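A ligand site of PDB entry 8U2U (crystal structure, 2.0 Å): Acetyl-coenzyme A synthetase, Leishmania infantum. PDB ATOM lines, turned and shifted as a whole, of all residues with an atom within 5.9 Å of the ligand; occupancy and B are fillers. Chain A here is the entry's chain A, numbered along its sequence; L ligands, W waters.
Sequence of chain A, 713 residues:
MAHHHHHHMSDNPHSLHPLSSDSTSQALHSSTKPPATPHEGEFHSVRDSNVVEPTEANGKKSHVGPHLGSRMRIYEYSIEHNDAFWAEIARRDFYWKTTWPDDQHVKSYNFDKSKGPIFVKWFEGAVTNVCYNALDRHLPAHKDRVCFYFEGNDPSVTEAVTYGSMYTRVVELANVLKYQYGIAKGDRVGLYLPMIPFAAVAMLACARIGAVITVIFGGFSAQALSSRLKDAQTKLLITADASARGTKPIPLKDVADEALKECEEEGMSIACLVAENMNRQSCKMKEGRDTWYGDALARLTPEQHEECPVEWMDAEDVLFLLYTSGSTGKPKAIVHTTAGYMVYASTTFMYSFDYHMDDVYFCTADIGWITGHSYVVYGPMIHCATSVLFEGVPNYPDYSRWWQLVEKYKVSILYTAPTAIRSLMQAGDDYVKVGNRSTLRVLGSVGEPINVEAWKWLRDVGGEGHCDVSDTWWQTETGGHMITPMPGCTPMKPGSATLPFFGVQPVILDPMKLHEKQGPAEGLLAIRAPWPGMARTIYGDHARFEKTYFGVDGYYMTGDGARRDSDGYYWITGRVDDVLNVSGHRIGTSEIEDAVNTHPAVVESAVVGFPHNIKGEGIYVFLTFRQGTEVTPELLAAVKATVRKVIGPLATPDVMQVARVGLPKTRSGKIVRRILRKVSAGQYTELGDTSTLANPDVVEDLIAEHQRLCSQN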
ATOM      1  N   MET A 195      -4.680 -13.269   3.847  1.00  0.00           N
ATOM      2  CA  MET A 195      -4.867 -14.161   5.005  1.00  0.00           C
ATOM      3  C   MET A 195      -6.353 -14.269   5.291  1.00  0.00           C
ATOM      4  O   MET A 195      -6.902 -13.588   6.162  1.00  0.00           O
ATOM      5  CB  MET A 195      -4.104 -13.644   6.245  1.00  0.00           C
ATOM      6  CG  MET A 195      -2.605 -13.661   6.055  1.00  0.00           C
ATOM      7  SD  MET A 195      -2.091 -15.378   5.931  1.00  0.00           S
ATOM      8  CE  MET A 195      -2.039 -15.670   7.714  1.00  0.00           C
ATOM      9  N   PHE A 217       3.752 -14.485  -1.543  1.00  0.00           N
ATOM     10  CA  PHE A 217       3.332 -13.414  -0.628  1.00  0.00           C
ATOM     11  C   PHE A 217       2.582 -12.291  -1.339  1.00  0.00           C
ATOM     12  O   PHE A 217       3.029 -11.770  -2.359  1.00  0.00           O
ATOM     13  CB  PHE A 217       4.614 -12.877   0.045  1.00  0.00           C
ATOM     14  CG  PHE A 217       4.417 -11.692   0.954  1.00  0.00           C
ATOM     15  CD1 PHE A 217       3.544 -11.756   2.028  1.00  0.00           C
ATOM     16  CD2 PHE A 217       5.171 -10.535   0.766  1.00  0.00           C
ATOM     17  CE1 PHE A 217       3.413 -10.655   2.896  1.00  0.00           C
ATOM     18  CE2 PHE A 217       5.022  -9.437   1.607  1.00  0.00           C
ATOM     19  CZ  PHE A 217       4.135  -9.509   2.678  1.00  0.00           C
ATOM     20  N   GLY A 218       1.450 -11.903  -0.774  1.00  0.00           N
ATOM     21  CA  GLY A 218       0.628 -10.872  -1.381  1.00  0.00           C
ATOM     22  C   GLY A 218       1.331  -9.538  -1.536  1.00  0.00           C
ATOM     23  O   GLY A 218       0.899  -8.710  -2.355  1.00  0.00           O
ATOM     24  N   GLY A 219       2.405  -9.302  -0.777  1.00  0.00           N
ATOM     25  CA  GLY A 219       3.208  -8.089  -0.952  1.00  0.00           C
ATOM     26  C   GLY A 219       4.105  -8.066  -2.198  1.00  0.00           C
ATOM     27  O   GLY A 219       4.661  -7.003  -2.512  1.00  0.00           O
ATOM     28  N   PHE A 220       4.257  -9.169  -2.908  1.00  0.00           N
ATOM     29  CA  PHE A 220       5.142  -9.189  -4.072  1.00  0.00           C
ATOM     30  C   PHE A 220       4.472  -8.487  -5.247  1.00  0.00           C
ATOM     31  O   PHE A 220       3.248  -8.461  -5.345  1.00  0.00           O
ATOM     32  CB  PHE A 220       5.532 -10.614  -4.476  1.00  0.00           C
ATOM     33  CG  PHE A 220       6.690 -11.170  -3.687  1.00  0.00           C
ATOM     34  CD1 PHE A 220       7.888 -10.472  -3.630  1.00  0.00           C
ATOM     35  CD2 PHE A 220       6.577 -12.350  -2.973  1.00  0.00           C
ATOM     36  CE1 PHE A 220       8.955 -10.952  -2.897  1.00  0.00           C
ATOM     37  CE2 PHE A 220       7.657 -12.837  -2.220  1.00  0.00           C
ATOM     38  CZ  PHE A 220       8.840 -12.135  -2.192  1.00  0.00           C
ATOM     39  N   ARG A 245      -5.177  -3.654   3.558  1.00  0.00           N
ATOM     40  CA  ARG A 245      -4.346  -3.590   4.760  1.00  0.00           C
ATOM     41  C   ARG A 245      -4.414  -2.176   5.302  1.00  0.00           C
ATOM     42  O   ARG A 245      -3.831  -1.258   4.725  1.00  0.00           O
ATOM     43  CB  ARG A 245      -2.913  -4.011   4.487  1.00  0.00           C
ATOM     44  CG  ARG A 245      -2.758  -5.525   4.401  1.00  0.00           C
ATOM     45  CD  ARG A 245      -1.313  -5.894   4.185  1.00  0.00           C
ATOM     46  NE  ARG A 245      -0.498  -5.711   5.392  1.00  0.00           N
ATOM     47  CZ  ARG A 245      -0.352  -6.646   6.324  1.00  0.00           C
ATOM     48  NH1 ARG A 245      -1.031  -7.772   6.282  1.00  0.00           N
ATOM     49  NH2 ARG A 245       0.532  -6.443   7.295  1.00  0.00           N
ATOM     50  N   LYS A 248      -4.976   0.981   2.896  1.00  0.00           N
ATOM     51  CA  LYS A 248      -4.368   0.771   1.581  1.00  0.00           C
ATOM     52  C   LYS A 248      -5.109  -0.344   0.850  1.00  0.00           C
ATOM     53  O   LYS A 248      -5.272  -1.434   1.403  1.00  0.00           O
ATOM     54  CB  LYS A 248      -2.895   0.395   1.718  1.00  0.00           C
ATOM     55  CG  LYS A 248      -2.232   0.010   0.379  1.00  0.00           C
ATOM     56  CD  LYS A 248      -0.769  -0.332   0.564  1.00  0.00           C
ATOM     57  CE  LYS A 248      -0.145  -0.808  -0.726  1.00  0.00           C
ATOM     58  NZ  LYS A 248       1.303  -1.117  -0.524  1.00  0.00           N
ATOM     59  N   ILE A 250      -5.290  -3.481  -1.448  1.00  0.00           N
ATOM     60  CA  ILE A 250      -4.316  -4.473  -1.880  1.00  0.00           C
ATOM     61  C   ILE A 250      -4.886  -5.091  -3.155  1.00  0.00           C
ATOM     62  O   ILE A 250      -5.737  -5.995  -3.093  1.00  0.00           O
ATOM     63  CB  ILE A 250      -4.020  -5.533  -0.822  1.00  0.00           C
ATOM     64  CG1 ILE A 250      -3.568  -4.885   0.515  1.00  0.00           C
ATOM     65  CG2 ILE A 250      -2.925  -6.461  -1.333  1.00  0.00           C
ATOM     66  CD1 ILE A 250      -2.222  -4.140   0.445  1.00  0.00           C
ATOM     67  N   ASP A 366       2.327 -14.245   7.788  1.00  0.00           N
ATOM     68  CA  ASP A 366       1.639 -14.469   6.529  1.00  0.00           C
ATOM     69  C   ASP A 366       1.971 -15.827   5.929  1.00  0.00           C
ATOM     70  O   ASP A 366       3.085 -16.338   6.100  1.00  0.00           O
ATOM     71  CB  ASP A 366       2.044 -13.355   5.553  1.00  0.00           C
ATOM     72  CG  ASP A 366       1.105 -13.240   4.369  1.00  0.00           C
ATOM     73  OD1 ASP A 366       1.265 -13.989   3.362  1.00  0.00           O
ATOM     74  OD2 ASP A 366       0.195 -12.371   4.456  1.00  0.00           O
ATOM     75  N   VAL A 393      -4.009  -5.539   9.905  1.00  0.00           N
ATOM     76  CA  VAL A 393      -2.741  -5.048  10.443  1.00  0.00           C
ATOM     77  C   VAL A 393      -2.952  -4.677  11.910  1.00  0.00           C
ATOM     78  O   VAL A 393      -4.075  -4.343  12.314  1.00  0.00           O
ATOM     79  CB  VAL A 393      -2.209  -3.834   9.659  1.00  0.00           C
ATOM     80  CG1 VAL A 393      -1.688  -4.270   8.327  1.00  0.00           C
ATOM     81  CG2 VAL A 393      -3.297  -2.765   9.498  1.00  0.00           C
ATOM     82  N   PRO A 394      -1.877  -4.689  12.695  1.00  0.00           N
ATOM     83  CA  PRO A 394      -2.007  -4.345  14.132  1.00  0.00           C
ATOM     84  C   PRO A 394      -2.451  -2.925  14.392  1.00  0.00           C
ATOM     85  O   PRO A 394      -2.815  -2.627  15.537  1.00  0.00           O
ATOM     86  CB  PRO A 394      -0.596  -4.598  14.678  1.00  0.00           C
ATOM     87  CG  PRO A 394       0.298  -4.476  13.482  1.00  0.00           C
ATOM     88  CD  PRO A 394      -0.486  -4.947  12.313  1.00  0.00           C
ATOM     89  N   ASN A 395      -2.424  -2.025  13.403  1.00  0.00           N
ATOM     90  CA  ASN A 395      -2.742  -0.634  13.696  1.00  0.00           C
ATOM     91  C   ASN A 395      -4.026  -0.155  13.034  1.00  0.00           C
ATOM     92  O   ASN A 395      -4.216   1.058  12.866  1.00  0.00           O
ATOM     93  CB  ASN A 395      -1.589   0.286  13.302  1.00  0.00           C
ATOM     94  CG  ASN A 395      -1.379   0.350  11.856  1.00  0.00           C
ATOM     95  OD1 ASN A 395      -1.580  -0.628  11.161  1.00  0.00           O
ATOM     96  ND2 ASN A 395      -0.974   1.508  11.368  1.00  0.00           N
ATOM     97  N   SER A 583      12.723  -6.196   8.814  1.00  0.00           N
ATOM     98  CA  SER A 583      11.447  -6.391   9.491  1.00  0.00           C
ATOM     99  C   SER A 583      11.079  -7.865   9.575  1.00  0.00           C
ATOM    100  O   SER A 583       9.895  -8.210   9.568  1.00  0.00           O
ATOM    101  CB  SER A 583      10.303  -5.641   8.806  1.00  0.00           C
ATOM    102  OG  SER A 583      10.595  -4.266   8.664  1.00  0.00           O
ATOM    103  N   HIS A 585      12.023 -10.115   7.295  1.00  0.00           N
ATOM    104  CA  HIS A 585      11.927 -10.650   5.952  1.00  0.00           C
ATOM    105  C   HIS A 585      13.318 -10.848   5.347  1.00  0.00           C
ATOM    106  O   HIS A 585      14.070  -9.876   5.201  1.00  0.00           O
ATOM    107  CB  HIS A 585      11.094  -9.721   5.072  1.00  0.00           C
ATOM    108  CG  HIS A 585       9.663  -9.634   5.503  1.00  0.00           C
ATOM    109  ND1 HIS A 585       8.943  -8.467   5.478  1.00  0.00           N
ATOM    110  CD2 HIS A 585       8.830 -10.579   5.995  1.00  0.00           C
ATOM    111  CE1 HIS A 585       7.722  -8.687   5.937  1.00  0.00           C
ATOM    112  NE2 HIS A 585       7.628  -9.963   6.247  1.00  0.00           N
ATOM    113  N   LYS A 615      12.869  -1.899  12.529  1.00  0.00           N
ATOM    114  CA  LYS A 615      12.934  -3.010  11.578  1.00  0.00           C
ATOM    115  C   LYS A 615      14.088  -3.966  11.827  1.00  0.00           C
ATOM    116  O   LYS A 615      14.224  -4.955  11.079  1.00  0.00           O
ATOM    117  CB  LYS A 615      13.049  -2.451  10.165  1.00  0.00           C
ATOM    118  CG  LYS A 615      12.118  -1.261   9.930  1.00  0.00           C
ATOM    119  CD  LYS A 615      11.610  -1.128   8.503  1.00  0.00           C
ATOM    120  CE  LYS A 615      12.684  -0.814   7.521  1.00  0.00           C
ATOM    121  NZ  LYS A 615      12.122  -0.767   6.113  1.00  0.00           N
ATOM    122  N   ARG A 644      10.220  -1.269  -5.880  1.00  0.00           N
ATOM    123  CA  ARG A 644       8.928  -1.772  -5.460  1.00  0.00           C
ATOM    124  C   ARG A 644       8.171  -2.425  -6.609  1.00  0.00           C
ATOM    125  O   ARG A 644       7.444  -3.400  -6.393  1.00  0.00           O
ATOM    126  CB  ARG A 644       8.137  -0.628  -4.824  1.00  0.00           C
ATOM    127  CG  ARG A 644       8.809  -0.111  -3.490  1.00  0.00           C
ATOM    128  CD  ARG A 644       8.205   1.195  -3.027  1.00  0.00           C
ATOM    129  NE  ARG A 644       6.755   1.148  -2.900  1.00  0.00           N
ATOM    130  CZ  ARG A 644       6.096   0.982  -1.758  1.00  0.00           C
ATOM    131  NH1 ARG A 644       6.713   0.779  -0.618  1.00  0.00           N
ATOM    132  NH2 ARG A 644       4.763   1.046  -1.766  1.00  0.00           N
ATOM    133  N   PRO A 649       6.950  -3.843  -2.061  1.00  0.00           N
ATOM    134  CA  PRO A 649       7.199  -2.866  -0.979  1.00  0.00           C
ATOM    135  C   PRO A 649       8.097  -3.363   0.141  1.00  0.00           C
ATOM    136  O   PRO A 649       8.764  -2.553   0.807  1.00  0.00           O
ATOM    137  CB  PRO A 649       5.780  -2.557  -0.461  1.00  0.00           C
ATOM    138  CG  PRO A 649       4.884  -2.852  -1.621  1.00  0.00           C
ATOM    139  CD  PRO A 649       5.506  -4.021  -2.324  1.00  0.00           C
ATOM    140  N   LEU A 650       8.136  -4.662   0.392  1.00  0.00           N
ATOM    141  CA  LEU A 650       9.016  -5.180   1.414  1.00  0.00           C
ATOM    142  C   LEU A 650      10.466  -4.821   1.135  1.00  0.00           C
ATOM    143  O   LEU A 650      11.273  -4.786   2.070  1.00  0.00           O
ATOM    144  CB  LEU A 650       8.875  -6.708   1.527  1.00  0.00           C
ATOM    145  CG  LEU A 650       9.250  -7.590   0.334  1.00  0.00           C
ATOM    146  CD1 LEU A 650       9.081  -9.052   0.710  1.00  0.00           C
ATOM    147  CD2 LEU A 650       8.452  -7.295  -0.957  1.00  0.00           C
ATOM    148  N   THR A 652      11.483  -1.921  -0.070  1.00  0.00           N
ATOM    149  CA  THR A 652      11.615  -0.480  -0.211  1.00  0.00           C
ATOM    150  C   THR A 652      12.882   0.038   0.483  1.00  0.00           C
ATOM    151  O   THR A 652      13.095  -0.234   1.676  1.00  0.00           O
ATOM    152  CB  THR A 652      10.404   0.242   0.364  1.00  0.00           C
ATOM    153  OG1 THR A 652       9.227  -0.199  -0.316  1.00  0.00           O
ATOM    154  CG2 THR A 652      10.575   1.738   0.195  1.00  0.00           C
HETATM  155  N1  LIG L   1       0.048  -8.039   1.207  1.00  0.00           N
HETATM  156  C1  LIG L   1       0.317  -6.982   0.486  1.00  0.00           C
HETATM  157  N2  LIG L   1       1.107  -6.036   0.944  1.00  0.00           N
HETATM  158  C2  LIG L   1       1.676  -6.164   2.177  1.00  0.00           C
HETATM  159  C3  LIG L   1       1.439  -7.253   2.960  1.00  0.00           C
HETATM  160  C4  LIG L   1       0.577  -8.228   2.425  1.00  0.00           C
HETATM  161  N3  LIG L   1       0.250  -9.417   3.190  1.00  0.00           N
HETATM  162  N4  LIG L   1       2.137  -7.110   4.108  1.00  0.00           N
HETATM  163  C5  LIG L   1       2.779  -5.954   4.022  1.00  0.00           C
HETATM  164  N5  LIG L   1       2.502  -5.377   2.863  1.00  0.00           N
HETATM  165  C6  LIG L   1       2.997  -4.093   2.344  1.00  0.00           C
HETATM  166  C7  LIG L   1       2.471  -2.906   3.207  1.00  0.00           C
HETATM  167  O1  LIG L   1       1.277  -2.522   2.695  1.00  0.00           O
HETATM  168  C8  LIG L   1       3.533  -1.867   3.039  1.00  0.00           C
HETATM  169  O2  LIG L   1       3.235  -1.127   1.820  1.00  0.00           O
HETATM  170  P1  LIG L   1       3.466   0.521   1.687  1.00  0.00           P
HETATM  171  O3  LIG L   1       4.928   0.832   1.614  1.00  0.00           O
HETATM  172  O4  LIG L   1       2.805   1.215   2.841  1.00  0.00           O
HETATM  173  O5  LIG L   1       2.798   0.977   0.429  1.00  0.00           O
HETATM  174  C9  LIG L   1       4.678  -2.567   2.839  1.00  0.00           C
HETATM  175  O6  LIG L   1       4.281  -4.058   2.449  1.00  0.00           O
HETATM  176  C10 LIG L   1       5.454  -2.706   4.137  1.00  0.00           C
HETATM  177  O7  LIG L   1       4.583  -3.372   5.053  1.00  0.00           O
HETATM  178  P2  LIG L   1       4.867  -3.066   6.693  1.00  0.00           P
HETATM  179  O8  LIG L   1       4.127  -1.786   7.088  1.00  0.00           O
HETATM  180  O9  LIG L   1       6.359  -2.944   6.825  1.00  0.00           O
HETATM  181  O10 LIG L   1       4.320  -4.298   7.650  1.00  0.00           O
HETATM  182  P3  LIG L   1       2.951  -3.888   8.471  1.00  0.00           P
HETATM  183  O11 LIG L   1       2.219  -3.197   7.386  1.00  0.00           O
HETATM  184  O12 LIG L   1       2.218  -5.093   8.959  1.00  0.00           O
HETATM  185  O13 LIG L   1       3.267  -2.955   9.642  1.00  0.00           O
HETATM  186  O   HOH W   1       3.501  -1.680  12.170  1.00  0.00           O
HETATM  187  O   HOH W   2       5.525  -5.173   9.830  1.00  0.00           O
HETATM  188  O   HOH W   3       2.682  -9.136   5.964  1.00  0.00           O
HETATM  189  O   HOH W   4       7.972  -1.005   3.321  1.00  0.00           O
HETATM  190  O   HOH W   5       1.464  -4.075  -0.905  1.00  0.00           O
HETATM  191  O   HOH W   6      -2.161  -9.815   0.800  1.00  0.00           O
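O12 of the ligand lies within salt-bridge range of NH2 of Arg 245 (2.7 Å). NZ of Lys 248 is in salt-bridge range of O5 of the ligand, 2.7 Å away. The guanidinium group (NH1) of Arg 644 is in salt-bridge range of an oxygen (O3) of the ligand (2.9 Å). The side-chain carboxylate of Asp 366 is in hydrogen-bond range of a nitrogen (N3) of the ligand, at 3.2 Å. N of Gly 219 is in hydrogen-bond range of N1 of the ligand (3.3 Å).
The side-chain hydroxyl (OG1) of Thr 652 lies within hydrogen-bond range of the guanidinium group (NH1) of Arg 644. The side-chain hydroxyl (OG1) of Thr 652 is in hydrogen-bond range of the backbone carbonyl oxygen (O) of Pro 649, 2.6 Å away.
CE1 of Phe 217 touches N3 of the ligand (3.4 Å). O of Gly 218 touches C1 of the ligand (3.4 Å). Ile 250 touches the ligand (CG2 to C1, 3.8 Å). Pro 649 touches the ligand (CB to C9, 3.5 Å). Hydrophobic or aromatic side chains that line the ligand: Phe 217, Ile 250 and Pro 649. Within 4 Å of the ligand: Phe 217, Gly 218, Gly 219, Arg 245, Lys 248, Ile 250, Asp 366, Arg 644 and Pro 649.
Water W5 bridges a nitrogen (N2) of the ligand (2.7 Å) and the side-chain amino group (NZ) of Lys 248 (3.0 Å).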
